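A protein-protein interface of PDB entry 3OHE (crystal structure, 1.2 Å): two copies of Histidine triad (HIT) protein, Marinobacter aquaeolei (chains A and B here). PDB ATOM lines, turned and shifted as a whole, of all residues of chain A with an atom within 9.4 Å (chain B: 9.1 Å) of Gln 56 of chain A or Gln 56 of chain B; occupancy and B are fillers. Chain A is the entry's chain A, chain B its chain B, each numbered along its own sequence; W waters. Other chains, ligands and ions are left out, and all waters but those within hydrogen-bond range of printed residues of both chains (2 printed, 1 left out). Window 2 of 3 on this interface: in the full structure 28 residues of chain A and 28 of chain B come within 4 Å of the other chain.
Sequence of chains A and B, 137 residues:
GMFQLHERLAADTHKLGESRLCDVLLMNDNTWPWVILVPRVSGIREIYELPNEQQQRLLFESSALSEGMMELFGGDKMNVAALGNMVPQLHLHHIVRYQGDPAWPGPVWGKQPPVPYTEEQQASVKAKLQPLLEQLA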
ATOM      1  N   LEU A  21      24.050   6.684 -34.498  1.00  0.00           N
ATOM      2  CA  LEU A  21      25.147   7.190 -33.682  1.00  0.00           C
ATOM      3  C   LEU A  21      26.142   6.133 -33.177  1.00  0.00           C
ATOM      4  O   LEU A  21      27.286   6.496 -32.880  1.00  0.00           O
ATOM      5  CB  LEU A  21      24.529   7.934 -32.475  1.00  0.00           C
ATOM      6  CG  LEU A  21      25.488   8.549 -31.439  1.00  0.00           C
ATOM      7  CD1 LEU A  21      26.326   9.645 -32.091  1.00  0.00           C
ATOM      8  CD2 LEU A  21      24.686   9.079 -30.253  1.00  0.00           C
ATOM      9  N   ILE A  47      28.250  10.182 -20.348  1.00  0.00           N
ATOM     10  CA  ILE A  47      27.141  10.659 -21.155  1.00  0.00           C
ATOM     11  C   ILE A  47      27.118  12.182 -21.263  1.00  0.00           C
ATOM     12  O   ILE A  47      26.912  12.730 -22.342  1.00  0.00           O
ATOM     13  CB  ILE A  47      25.764  10.139 -20.630  1.00  0.00           C
ATOM     14  CG1 ILE A  47      25.683   8.620 -20.700  1.00  0.00           C
ATOM     15  CG2 ILE A  47      24.575  10.851 -21.364  1.00  0.00           C
ATOM     16  CD1 ILE A  47      24.599   8.054 -19.750  1.00  0.00           C
ATOM     17  N   TYR A  48      27.376  12.839 -20.136  1.00  0.00           N
ATOM     18  CA  TYR A  48      27.288  14.277 -20.085  1.00  0.00           C
ATOM     19  C   TYR A  48      28.341  14.995 -20.945  1.00  0.00           C
ATOM     20  O   TYR A  48      28.229  16.217 -21.164  1.00  0.00           O
ATOM     21  CB  TYR A  48      27.307  14.779 -18.618  1.00  0.00           C
ATOM     22  CG  TYR A  48      28.598  14.549 -17.874  1.00  0.00           C
ATOM     23  CD1 TYR A  48      29.723  15.349 -18.081  1.00  0.00           C
ATOM     24  CD2 TYR A  48      28.682  13.598 -16.893  1.00  0.00           C
ATOM     25  CE1 TYR A  48      30.874  15.129 -17.374  1.00  0.00           C
ATOM     26  CE2 TYR A  48      29.821  13.398 -16.163  1.00  0.00           C
ATOM     27  CZ  TYR A  48      30.903  14.159 -16.402  1.00  0.00           C
ATOM     28  OH  TYR A  48      32.036  13.956 -15.672  1.00  0.00           O
ATOM     29  N   LEU A  50      28.979  14.229 -24.064  1.00  0.00           N
ATOM     30  CA  LEU A  50      28.485  14.324 -25.430  1.00  0.00           C
ATOM     31  C   LEU A  50      27.803  15.695 -25.592  1.00  0.00           C
ATOM     32  O   LEU A  50      27.156  16.194 -24.682  1.00  0.00           O
ATOM     33  CB  LEU A  50      27.455  13.250 -25.713  1.00  0.00           C
ATOM     34  CG  LEU A  50      27.949  11.826 -25.894  1.00  0.00           C
ATOM     35  CD1 LEU A  50      26.738  10.892 -25.894  1.00  0.00           C
ATOM     36  CD2 LEU A  50      28.751  11.651 -27.203  1.00  0.00           C
ATOM     37  N   PRO A  51      27.931  16.302 -26.782  1.00  0.00           N
ATOM     38  CA  PRO A  51      27.087  17.431 -27.109  1.00  0.00           C
ATOM     39  C   PRO A  51      25.601  17.131 -26.856  1.00  0.00           C
ATOM     40  O   PRO A  51      25.157  15.999 -27.028  1.00  0.00           O
ATOM     41  CB  PRO A  51      27.338  17.629 -28.620  1.00  0.00           C
ATOM     42  CG  PRO A  51      28.673  17.025 -28.884  1.00  0.00           C
ATOM     43  CD  PRO A  51      28.782  15.882 -27.907  1.00  0.00           C
ATOM     44  N   ASN A  52      24.819  18.138 -26.494  1.00  0.00           N
ATOM     45  CA  ASN A  52      23.442  17.926 -26.085  1.00  0.00           C
ATOM     46  C   ASN A  52      22.656  17.143 -27.128  1.00  0.00           C
ATOM     47  O   ASN A  52      21.927  16.238 -26.770  1.00  0.00           O
ATOM     48  CB  ASN A  52      22.683  19.240 -25.780  1.00  0.00           C
ATOM     49  CG  ASN A  52      21.354  18.966 -25.048  1.00  0.00           C
ATOM     50  OD1 ASN A  52      20.295  19.277 -25.561  1.00  0.00           O
ATOM     51  ND2 ASN A  52      21.421  18.329 -23.870  1.00  0.00           N
ATOM     52  N   GLU A  53      22.803  17.476 -28.412  1.00  0.00           N
ATOM     53  CA  GLU A  53      22.021  16.763 -29.435  1.00  0.00           C
ATOM     54  C   GLU A  53      22.403  15.291 -29.527  1.00  0.00           C
ATOM     55  O   GLU A  53      21.552  14.446 -29.835  1.00  0.00           O
ATOM     56  CB  GLU A  53      22.157  17.425 -30.807  1.00  0.00           C
ATOM     57  CG  GLU A  53      21.538  18.807 -30.871  1.00  0.00           C
ATOM     58  CD  GLU A  53      20.008  18.812 -30.798  1.00  0.00           C
ATOM     59  OE1 GLU A  53      19.308  17.759 -30.955  1.00  0.00           O
ATOM     60  OE2 GLU A  53      19.478  19.913 -30.572  1.00  0.00           O
ATOM     61  N   GLN A  54      23.676  14.991 -29.275  1.00  0.00           N
ATOM     62  CA  GLN A  54      24.114  13.606 -29.285  1.00  0.00           C
ATOM     63  C   GLN A  54      23.684  12.864 -28.051  1.00  0.00           C
ATOM     64  O   GLN A  54      23.321  11.677 -28.138  1.00  0.00           O
ATOM     65  CB  GLN A  54      25.628  13.496 -29.523  1.00  0.00           C
ATOM     66  CG  GLN A  54      26.008  13.970 -30.923  1.00  0.00           C
ATOM     67  CD  GLN A  54      27.488  14.045 -31.171  1.00  0.00           C
ATOM     68  OE1 GLN A  54      28.284  13.777 -30.308  1.00  0.00           O
ATOM     69  NE2 GLN A  54      27.850  14.516 -32.335  1.00  0.00           N
ATOM     70  N   GLN A  55      23.600  13.562 -26.916  1.00  0.00           N
ATOM     71  CA  GLN A  55      22.939  12.943 -25.770  1.00  0.00           C
ATOM     72  C   GLN A  55      21.488  12.550 -26.080  1.00  0.00           C
ATOM     73  O   GLN A  55      21.023  11.465 -25.716  1.00  0.00           O
ATOM     74  CB  GLN A  55      22.940  13.852 -24.534  1.00  0.00           C
ATOM     75  CG  GLN A  55      24.307  14.167 -23.965  1.00  0.00           C
ATOM     76  CD  GLN A  55      24.228  15.015 -22.712  1.00  0.00           C
ATOM     77  OE1 GLN A  55      23.316  14.820 -21.881  1.00  0.00           O
ATOM     78  NE2 GLN A  55      25.141  15.971 -22.563  1.00  0.00           N
ATOM     79  N   GLN A  56      20.772  13.466 -26.719  1.00  0.00           N
ATOM     80  CA  GLN A  56      19.375  13.199 -27.047  1.00  0.00           C
ATOM     81  C   GLN A  56      19.226  12.082 -28.093  1.00  0.00           C
ATOM     82  O   GLN A  56      18.289  11.309 -28.016  1.00  0.00           O
ATOM     83  CB  GLN A  56      18.664  14.471 -27.491  1.00  0.00           C
ATOM     84  CG  GLN A  56      18.460  15.483 -26.354  1.00  0.00           C
ATOM     85  CD  GLN A  56      17.631  16.663 -26.780  1.00  0.00           C
ATOM     86  OE1 GLN A  56      17.438  16.897 -27.993  1.00  0.00           O
ATOM     87  NE2 GLN A  56      17.095  17.403 -25.807  1.00  0.00           N
ATOM     88  N   ARG A  57      20.151  11.970 -29.032  1.00  0.00           N
ATOM     89  CA  ARG A  57      20.126  10.856 -29.959  1.00  0.00           C
ATOM     90  C   ARG A  57      20.413   9.536 -29.256  1.00  0.00           C
ATOM     91  O   ARG A  57      19.746   8.529 -29.525  1.00  0.00           O
ATOM     92  CB  ARG A  57      21.085  11.089 -31.126  1.00  0.00           C
ATOM     93  CG  ARG A  57      21.107   9.956 -32.157  1.00  0.00           C
ATOM     94  CD  ARG A  57      19.821   9.873 -32.942  1.00  0.00           C
ATOM     95  NE  ARG A  57      19.718   8.584 -33.614  1.00  0.00           N
ATOM     96  CZ  ARG A  57      18.684   8.246 -34.364  1.00  0.00           C
ATOM     97  NH1 ARG A  57      17.752   9.136 -34.695  1.00  0.00           N
ATOM     98  NH2 ARG A  57      18.616   7.013 -34.817  1.00  0.00           N
ATOM     99  N   LEU A  58      21.387   9.534 -28.363  1.00  0.00           N
ATOM    100  CA  LEU A  58      21.675   8.335 -27.597  1.00  0.00           C
ATOM    101  C   LEU A  58      20.457   7.896 -26.782  1.00  0.00           C
ATOM    102  O   LEU A  58      20.145   6.716 -26.710  1.00  0.00           O
ATOM    103  CB  LEU A  58      22.876   8.556 -26.658  1.00  0.00           C
ATOM    104  CG  LEU A  58      23.317   7.355 -25.812  1.00  0.00           C
ATOM    105  CD1 LEU A  58      23.633   6.127 -26.694  1.00  0.00           C
ATOM    106  CD2 LEU A  58      24.506   7.789 -24.956  1.00  0.00           C
ATOM    107  N   LEU A  59      19.780   8.854 -26.145  1.00  0.00           N
ATOM    108  CA  LEU A  59      18.565   8.550 -25.410  1.00  0.00           C
ATOM    109  C   LEU A  59      17.503   7.936 -26.307  1.00  0.00           C
ATOM    110  O   LEU A  59      16.859   6.941 -25.963  1.00  0.00           O
ATOM    111  CB  LEU A  59      18.030   9.829 -24.741  1.00  0.00           C
ATOM    112  CG  LEU A  59      16.629   9.760 -24.146  1.00  0.00           C
ATOM    113  CD1 LEU A  59      16.559   8.796 -22.960  1.00  0.00           C
ATOM    114  CD2 LEU A  59      16.159  11.212 -23.748  1.00  0.00           C
ATOM    115  N   PHE A  60      17.275   8.545 -27.471  1.00  0.00           N
ATOM    116  CA  PHE A  60      16.286   8.006 -28.430  1.00  0.00           C
ATOM    117  C   PHE A  60      16.627   6.542 -28.749  1.00  0.00           C
ATOM    118  O   PHE A  60      15.756   5.659 -28.701  1.00  0.00           O
ATOM    119  CB  PHE A  60      16.244   8.842 -29.725  1.00  0.00           C
ATOM    120  CG  PHE A  60      15.487   8.183 -30.807  1.00  0.00           C
ATOM    121  CD1 PHE A  60      14.115   8.160 -30.801  1.00  0.00           C
ATOM    122  CD2 PHE A  60      16.154   7.445 -31.787  1.00  0.00           C
ATOM    123  CE1 PHE A  60      13.420   7.491 -31.831  1.00  0.00           C
ATOM    124  CE2 PHE A  60      15.469   6.767 -32.789  1.00  0.00           C
ATOM    125  CZ  PHE A  60      14.099   6.788 -32.782  1.00  0.00           C
ATOM    126  N   GLU A  61      17.881   6.294 -29.088  1.00  0.00           N
ATOM    127  CA  GLU A  61      18.306   4.947 -29.486  1.00  0.00           C
ATOM    128  C   GLU A  61      18.193   3.972 -28.321  1.00  0.00           C
ATOM    129  O   GLU A  61      17.736   2.831 -28.494  1.00  0.00           O
ATOM    130  CB  GLU A  61      19.738   4.960 -30.051  1.00  0.00           C
ATOM    131  CG  GLU A  61      19.802   5.756 -31.364  1.00  0.00           C
ATOM    132  CD  GLU A  61      21.163   5.722 -32.057  1.00  0.00           C
ATOM    133  OE1 GLU A  61      22.057   5.079 -31.499  1.00  0.00           O
ATOM    134  OE2 GLU A  61      21.317   6.331 -33.151  1.00  0.00           O
ATOM    135  N   SER A  62      18.629   4.378 -27.143  1.00  0.00           N
ATOM    136  CA  SER A  62      18.606   3.528 -25.956  1.00  0.00           C
ATOM    137  C   SER A  62      17.184   3.163 -25.565  1.00  0.00           C
ATOM    138  O   SER A  62      16.885   1.999 -25.266  1.00  0.00           O
ATOM    139  CB  SER A  62      19.283   4.235 -24.798  1.00  0.00           C
ATOM    140  OG  SER A  62      19.221   3.464 -23.612  1.00  0.00           O
ATOM    141  N   SER A  63      16.295   4.163 -25.539  1.00  0.00           N
ATOM    142  CA  SER A  63      14.896   3.898 -25.202  1.00  0.00           C
ATOM    143  C   SER A  63      14.237   2.990 -26.220  1.00  0.00           C
ATOM    144  O   SER A  63      13.446   2.097 -25.857  1.00  0.00           O
ATOM    145  CB  SER A  63      14.132   5.194 -25.061  1.00  0.00           C
ATOM    146  OG  SER A  63      14.444   5.781 -23.812  1.00  0.00           O
ATOM    147  N   ALA A  64      14.512   3.160 -27.504  1.00  0.00           N
ATOM    148  CA  ALA A  64      13.925   2.328 -28.558  1.00  0.00           C
ATOM    149  C   ALA A  64      14.479   0.901 -28.447  1.00  0.00           C
ATOM    150  O   ALA A  64      13.742  -0.100 -28.526  1.00  0.00           O
ATOM    151  CB  ALA A  64      14.193   2.926 -29.957  1.00  0.00           C
ATOM    152  N   ARG B  20      12.990  19.905 -11.414  1.00  0.00           N
ATOM    153  CA  ARG B  20      11.789  20.187 -12.208  1.00  0.00           C
ATOM    154  C   ARG B  20      10.907  18.944 -12.369  1.00  0.00           C
ATOM    155  O   ARG B  20       9.691  19.027 -12.247  1.00  0.00           O
ATOM    156  CB  ARG B  20      12.156  20.739 -13.600  1.00  0.00           C
ATOM    157  CG  ARG B  20      11.045  21.569 -14.220  1.00  0.00           C
ATOM    158  CD  ARG B  20      11.424  22.158 -15.535  1.00  0.00           C
ATOM    159  NE  ARG B  20      12.537  23.046 -15.364  1.00  0.00           N
ATOM    160  CZ  ARG B  20      13.230  23.587 -16.364  1.00  0.00           C
ATOM    161  NH1 ARG B  20      12.875  23.386 -17.638  1.00  0.00           N
ATOM    162  NH2 ARG B  20      14.272  24.341 -16.094  1.00  0.00           N
ATOM    163  N   LEU B  21      11.533  17.789 -12.560  1.00  0.00           N
ATOM    164  CA  LEU B  21      10.854  16.539 -12.822  1.00  0.00           C
ATOM    165  C   LEU B  21      10.834  15.557 -11.643  1.00  0.00           C
ATOM    166  O   LEU B  21       9.920  14.725 -11.591  1.00  0.00           O
ATOM    167  CB  LEU B  21      11.499  15.863 -14.037  1.00  0.00           C
ATOM    168  CG  LEU B  21      10.909  14.530 -14.494  1.00  0.00           C
ATOM    169  CD1 LEU B  21       9.457  14.602 -14.900  1.00  0.00           C
ATOM    170  CD2 LEU B  21      11.772  13.938 -15.607  1.00  0.00           C
ATOM    171  N   ILE B  47      12.627   4.001 -18.235  1.00  0.00           N
ATOM    172  CA  ILE B  47      12.795   5.327 -18.821  1.00  0.00           C
ATOM    173  C   ILE B  47      11.911   5.492 -20.062  1.00  0.00           C
ATOM    174  O   ILE B  47      11.313   6.544 -20.279  1.00  0.00           O
ATOM    175  CB  ILE B  47      14.283   5.591 -19.171  1.00  0.00           C
ATOM    176  CG1 ILE B  47      15.148   5.645 -17.906  1.00  0.00           C
ATOM    177  CG2 ILE B  47      14.431   6.909 -20.005  1.00  0.00           C
ATOM    178  CD1 ILE B  47      16.635   5.540 -18.239  1.00  0.00           C
ATOM    179  N   LEU B  50       8.245   6.968 -20.047  1.00  0.00           N
ATOM    180  CA  LEU B  50       7.953   8.388 -19.915  1.00  0.00           C
ATOM    181  C   LEU B  50       7.609   8.945 -21.300  1.00  0.00           C
ATOM    182  O   LEU B  50       8.192   8.542 -22.315  1.00  0.00           O
ATOM    183  CB  LEU B  50       9.155   9.136 -19.328  1.00  0.00           C
ATOM    184  CG  LEU B  50       9.478   8.889 -17.865  1.00  0.00           C
ATOM    185  CD1 LEU B  50      10.857   9.438 -17.553  1.00  0.00           C
ATOM    186  CD2 LEU B  50       8.421   9.485 -16.932  1.00  0.00           C
ATOM    187  N   PRO B  51       6.758   9.981 -21.333  1.00  0.00           N
ATOM    188  CA  PRO B  51       6.647  10.743 -22.561  1.00  0.00           C
ATOM    189  C   PRO B  51       8.005  11.321 -23.015  1.00  0.00           C
ATOM    190  O   PRO B  51       8.886  11.579 -22.173  1.00  0.00           O
ATOM    191  CB  PRO B  51       5.739  11.907 -22.171  1.00  0.00           C
ATOM    192  CG  PRO B  51       5.092  11.591 -20.928  1.00  0.00           C
ATOM    193  CD  PRO B  51       5.938  10.541 -20.252  1.00  0.00           C
ATOM    194  N   ASN B  52       8.203  11.468 -24.314  1.00  0.00           N
ATOM    195  CA  ASN B  52       9.526  11.822 -24.824  1.00  0.00           C
ATOM    196  C   ASN B  52      10.125  13.060 -24.178  1.00  0.00           C
ATOM    197  O   ASN B  52      11.295  13.119 -23.887  1.00  0.00           O
ATOM    198  CB  ASN B  52       9.487  11.999 -26.342  1.00  0.00           C
ATOM    199  CG  ASN B  52       9.230  10.707 -27.082  1.00  0.00           C
ATOM    200  OD1 ASN B  52       9.662   9.622 -26.663  1.00  0.00           O
ATOM    201  ND2 ASN B  52       8.566  10.821 -28.241  1.00  0.00           N
ATOM    202  N   GLU B  53       9.295  14.053 -23.913  1.00  0.00           N
ATOM    203  CA  GLU B  53       9.778  15.299 -23.334  1.00  0.00           C
ATOM    204  C   GLU B  53      10.212  15.131 -21.883  1.00  0.00           C
ATOM    205  O   GLU B  53      11.136  15.811 -21.443  1.00  0.00           O
ATOM    206  CB  GLU B  53       8.738  16.410 -23.487  1.00  0.00           C
ATOM    207  CG  GLU B  53       7.575  16.352 -22.512  1.00  0.00           C
ATOM    208  CD  GLU B  53       6.573  17.487 -22.730  1.00  0.00           C
ATOM    209  OE1 GLU B  53       5.868  17.470 -23.766  1.00  0.00           O
ATOM    210  OE2 GLU B  53       6.486  18.391 -21.863  1.00  0.00           O
ATOM    211  N   GLN B  54       9.558  14.256 -21.131  1.00  0.00           N
ATOM    212  CA  GLN B  54      10.038  13.902 -19.786  1.00  0.00           C
ATOM    213  C   GLN B  54      11.285  13.030 -19.840  1.00  0.00           C
ATOM    214  O   GLN B  54      12.149  13.166 -18.973  1.00  0.00           O
ATOM    215  CB  GLN B  54       8.918  13.267 -18.950  1.00  0.00           C
ATOM    216  CG  GLN B  54       7.861  14.281 -18.622  1.00  0.00           C
ATOM    217  CD  GLN B  54       6.760  13.772 -17.726  1.00  0.00           C
ATOM    218  OE1 GLN B  54       6.399  12.603 -17.775  1.00  0.00           O
ATOM    219  NE2 GLN B  54       6.170  14.665 -16.929  1.00  0.00           N
ATOM    220  N   GLN B  55      11.418  12.138 -20.828  1.00  0.00           N
ATOM    221  CA  GLN B  55      12.689  11.420 -21.008  1.00  0.00           C
ATOM    222  C   GLN B  55      13.813  12.434 -21.218  1.00  0.00           C
ATOM    223  O   GLN B  55      14.889  12.308 -20.600  1.00  0.00           O
ATOM    224  CB  GLN B  55      12.669  10.469 -22.203  1.00  0.00           C
ATOM    225  CG  GLN B  55      11.712   9.312 -22.080  1.00  0.00           C
ATOM    226  CD  GLN B  55      11.820   8.358 -23.242  1.00  0.00           C
ATOM    227  OE1 GLN B  55      12.947   8.124 -23.750  1.00  0.00           O
ATOM    228  NE2 GLN B  55      10.687   7.827 -23.698  1.00  0.00           N
ATOM    229  N   GLN B  56      13.579  13.425 -22.071  1.00  0.00           N
ATOM    230  CA  GLN B  56      14.620  14.405 -22.366  1.00  0.00           C
ATOM    231  C   GLN B  56      14.923  15.274 -21.144  1.00  0.00           C
ATOM    232  O   GLN B  56      16.063  15.665 -20.939  1.00  0.00           O
ATOM    233  CB  GLN B  56      14.249  15.253 -23.593  1.00  0.00           C
ATOM    234  CG  GLN B  56      14.127  14.460 -24.893  1.00  0.00           C
ATOM    235  CD  GLN B  56      14.162  15.351 -26.108  1.00  0.00           C
ATOM    236  OE1 GLN B  56      13.811  16.527 -26.030  1.00  0.00           O
ATOM    237  NE2 GLN B  56      14.599  14.801 -27.231  1.00  0.00           N
ATOM    238  N   ARG B  57      13.912  15.590 -20.339  1.00  0.00           N
ATOM    239  CA  ARG B  57      14.177  16.349 -19.136  1.00  0.00           C
ATOM    240  C   ARG B  57      14.968  15.514 -18.107  1.00  0.00           C
ATOM    241  O   ARG B  57      15.898  16.019 -17.456  1.00  0.00           O
ATOM    242  CB  ARG B  57      12.899  16.906 -18.495  1.00  0.00           C
ATOM    243  CG  ARG B  57      13.154  17.686 -17.204  1.00  0.00           C
ATOM    244  CD  ARG B  57      13.910  18.967 -17.445  1.00  0.00           C
ATOM    245  NE  ARG B  57      14.401  19.527 -16.187  1.00  0.00           N
ATOM    246  CZ  ARG B  57      15.197  20.591 -16.131  1.00  0.00           C
ATOM    247  NH1 ARG B  57      15.508  21.264 -17.213  1.00  0.00           N
ATOM    248  NH2 ARG B  57      15.691  20.963 -14.965  1.00  0.00           N
ATOM    249  N   LEU B  58      14.627  14.234 -17.961  1.00  0.00           N
ATOM    250  CA  LEU B  58      15.361  13.343 -17.069  1.00  0.00           C
ATOM    251  C   LEU B  58      16.827  13.288 -17.502  1.00  0.00           C
ATOM    252  O   LEU B  58      17.723  13.331 -16.659  1.00  0.00           O
ATOM    253  CB  LEU B  58      14.756  11.941 -17.059  1.00  0.00           C
ATOM    254  CG  LEU B  58      15.456  10.914 -16.176  1.00  0.00           C
ATOM    255  CD1 LEU B  58      15.554  11.342 -14.710  1.00  0.00           C
ATOM    256  CD2 LEU B  58      14.743   9.567 -16.334  1.00  0.00           C
ATOM    257  N   LEU B  59      17.073  13.125 -18.798  1.00  0.00           N
ATOM    258  CA  LEU B  59      18.439  13.148 -19.341  1.00  0.00           C
ATOM    259  C   LEU B  59      19.176  14.435 -18.978  1.00  0.00           C
ATOM    260  O   LEU B  59      20.330  14.403 -18.532  1.00  0.00           O
ATOM    261  CB  LEU B  59      18.402  12.963 -20.867  1.00  0.00           C
ATOM    262  CG  LEU B  59      19.693  13.250 -21.617  1.00  0.00           C
ATOM    263  CD1 LEU B  59      20.764  12.228 -21.233  1.00  0.00           C
ATOM    264  CD2 LEU B  59      19.436  13.317 -23.148  1.00  0.00           C
ATOM    265  N   PHE B  60      18.542  15.579 -19.186  1.00  0.00           N
ATOM    266  CA  PHE B  60      19.170  16.823 -18.847  1.00  0.00           C
ATOM    267  C   PHE B  60      19.556  16.876 -17.366  1.00  0.00           C
ATOM    268  O   PHE B  60      20.677  17.282 -17.023  1.00  0.00           O
ATOM    269  CB  PHE B  60      18.270  18.010 -19.205  1.00  0.00           C
ATOM    270  CG  PHE B  60      18.850  19.337 -18.733  1.00  0.00           C
ATOM    271  CD1 PHE B  60      19.773  20.017 -19.514  1.00  0.00           C
ATOM    272  CD2 PHE B  60      18.564  19.825 -17.469  1.00  0.00           C
ATOM    273  CE1 PHE B  60      20.349  21.226 -19.065  1.00  0.00           C
ATOM    274  CE2 PHE B  60      19.144  21.001 -17.003  1.00  0.00           C
ATOM    275  CZ  PHE B  60      20.031  21.689 -17.805  1.00  0.00           C
ATOM    276  N   GLU B  61      18.625  16.520 -16.498  1.00  0.00           N
ATOM    277  CA  GLU B  61      18.851  16.568 -15.091  1.00  0.00           C
ATOM    278  C   GLU B  61      19.951  15.587 -14.685  1.00  0.00           C
ATOM    279  O   GLU B  61      20.815  15.910 -13.859  1.00  0.00           O
ATOM    280  CB  GLU B  61      17.585  16.295 -14.282  1.00  0.00           C
ATOM    281  CG  GLU B  61      16.520  17.382 -14.447  1.00  0.00           C
ATOM    282  CD  GLU B  61      15.254  17.198 -13.632  1.00  0.00           C
ATOM    283  OE1 GLU B  61      15.217  16.212 -12.867  1.00  0.00           O
ATOM    284  OE2 GLU B  61      14.347  18.105 -13.766  1.00  0.00           O
ATOM    285  N   SER B  62      19.909  14.377 -15.233  1.00  0.00           N
ATOM    286  CA  SER B  62      20.930  13.360 -14.945  1.00  0.00           C
ATOM    287  C   SER B  62      22.331  13.840 -15.353  1.00  0.00           C
ATOM    288  O   SER B  62      23.289  13.719 -14.608  1.00  0.00           O
ATOM    289  CB  SER B  62      20.601  12.077 -15.686  1.00  0.00           C
ATOM    290  OG  SER B  62      21.610  11.108 -15.547  1.00  0.00           O
ATOM    291  N   SER B  63      22.450  14.396 -16.550  1.00  0.00           N
ATOM    292  CA  SER B  63      23.741  14.878 -17.015  1.00  0.00           C
ATOM    293  C   SER B  63      24.242  16.084 -16.212  1.00  0.00           C
ATOM    294  O   SER B  63      25.457  16.178 -15.943  1.00  0.00           O
ATOM    295  CB  SER B  63      23.679  15.210 -18.495  1.00  0.00           C
ATOM    296  OG  SER B  63      23.679  13.987 -19.242  1.00  0.00           O
ATOM    297  N   ALA B  64      23.349  16.972 -15.787  1.00  0.00           N
ATOM    298  CA  ALA B  64      23.713  18.118 -14.980  1.00  0.00           C
ATOM    299  C   ALA B  64      24.171  17.654 -13.609  1.00  0.00           C
ATOM    300  O   ALA B  64      25.198  18.084 -13.073  1.00  0.00           O
ATOM    301  CB  ALA B  64      22.527  19.110 -14.870  1.00  0.00           C
HETATM  302  O   HOH W   1      15.728  12.227 -27.343  1.00  0.00           O
HETATM  303  O   HOH W   2      17.765  16.516 -23.036  1.00  0.00           O
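Among the printed residues, merely in contact across the chains: Tyr 48 of chain A with Ser 63 of chain B (3.5 Å), Gln 55 of chain A with Leu 59 of chain B (3.5 Å), Leu 59 of chain A with Gln 55 of chain B (3.6 Å), Leu 59 of chain A with Gln 56 of chain B (3.8 Å), Gln 56 of chain A with Leu 59 of chain B (3.8 Å), Ile 47 of chain A with Ser 63 of chain B (3.9 Å), Leu 59 of chain A with Leu 59 of chain B (3.9 Å) and Ser 63 of chain A with Ile 47 of chain B (3.97 Å).
The backbone carbonyl oxygen (O) of Leu 50 of chain A lies within hydrogen-bond range of the side-chain amide nitrogen (NE2) of Gln 55 of chain A. The backbone carbonyl oxygen (O) of Leu 59 of chain A lies close to the side-chain hydroxyl (OG) of Ser 63 of chain A. The side-chain hydroxyl of Ser 63 of chain B lies close to the backbone carbonyl oxygen of Leu 59 of chain B.
Ile 47 of chain A touches Ser 63 of chain B, and with the chains exchanged Ser 63 of chain A touches Ile 47 of chain B. Gln 55 of chain A touches Leu 59 of chain B, and with the chains exchanged Leu 59 of chain A touches Gln 55 of chain B. Leu 59 of chain B touches its own counterpart, Leu 59 of chain A. 17 positions are printed for both chains. Of the 11 pairs that touch across the chains among the printed residues, 10 have their exchanged pair printed and touching as well.
Water W1 bridges the backbone carbonyl oxygen of Gln 56 of chain A (2.8 Å) and the side-chain amide nitrogen of Gln 56 of chain B (2.8 Å). Water W2 lies within hydrogen-bond range of O of Gln 56 of chain B (2.8 Å) and NE2 of Gln 56 of chain A (3.0 Å).
Printed residues of chain B within 4 Å of Ile 47 of chain A: Ser 63. Printed residues of chain B within 4 Å of Gln 56 of chain A: Gln 56 and Leu 59. Ser 62 of chain A touches none of the printed residues of chain B. Of the printed residues of chain A, Leu 59 of chain B touches Gln 55 (3.5 Å), Gln 56 (3.8 Å) and Leu 59 (3.9 Å). Ser 62 of chain B touches none of the printed residues of chain A. Of the printed residues of chain A, Ser 63 of chain B touches Ile 47 (3.9 Å), Tyr 48 (3.5 Å) and Gln 55 (2.8 Å). The nearest printed residue of chain B that does not touch Gln 56 of chain A is Arg 57 of chain B (6.6 Å).
The side-chain hydroxyl (OG) of Ser 63 of chain B lies within hydrogen-bond range of the side-chain amide oxygen (OE1) of Gln 55 of chain A (2.8 Å). OE1 of Gln 56 of chain B is in hydrogen-bond range of NE2 of Gln 56 of chain A (3.4 Å). OG of Ser 63 of chain A is in hydrogen-bond range of OE1 of Gln 55 of chain B (2.8 Å).
Printed residues of chain B that touch a printed residue of chain A: Ile 47, Gln 55, Gln 56, Leu 59 and Ser 63. Hydrophobic or aromatic side chains of chain B within 4 Å of the printed part of chain A: Ile 47 and Leu 59. Printed residues of chain A that touch a printed residue of chain B: Ile 47, Tyr 48, Gln 55, Gln 56, Leu 59 and Ser 63. Hydrophobic or aromatic side chains of chain A that line the printed part of chain B: Ile 47, Tyr 48 and Leu 59. Among the printed residues, no Asp or Glu carboxylate lies within 4 Å of a Lys or Arg side-chain nitrogen of the other chain.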
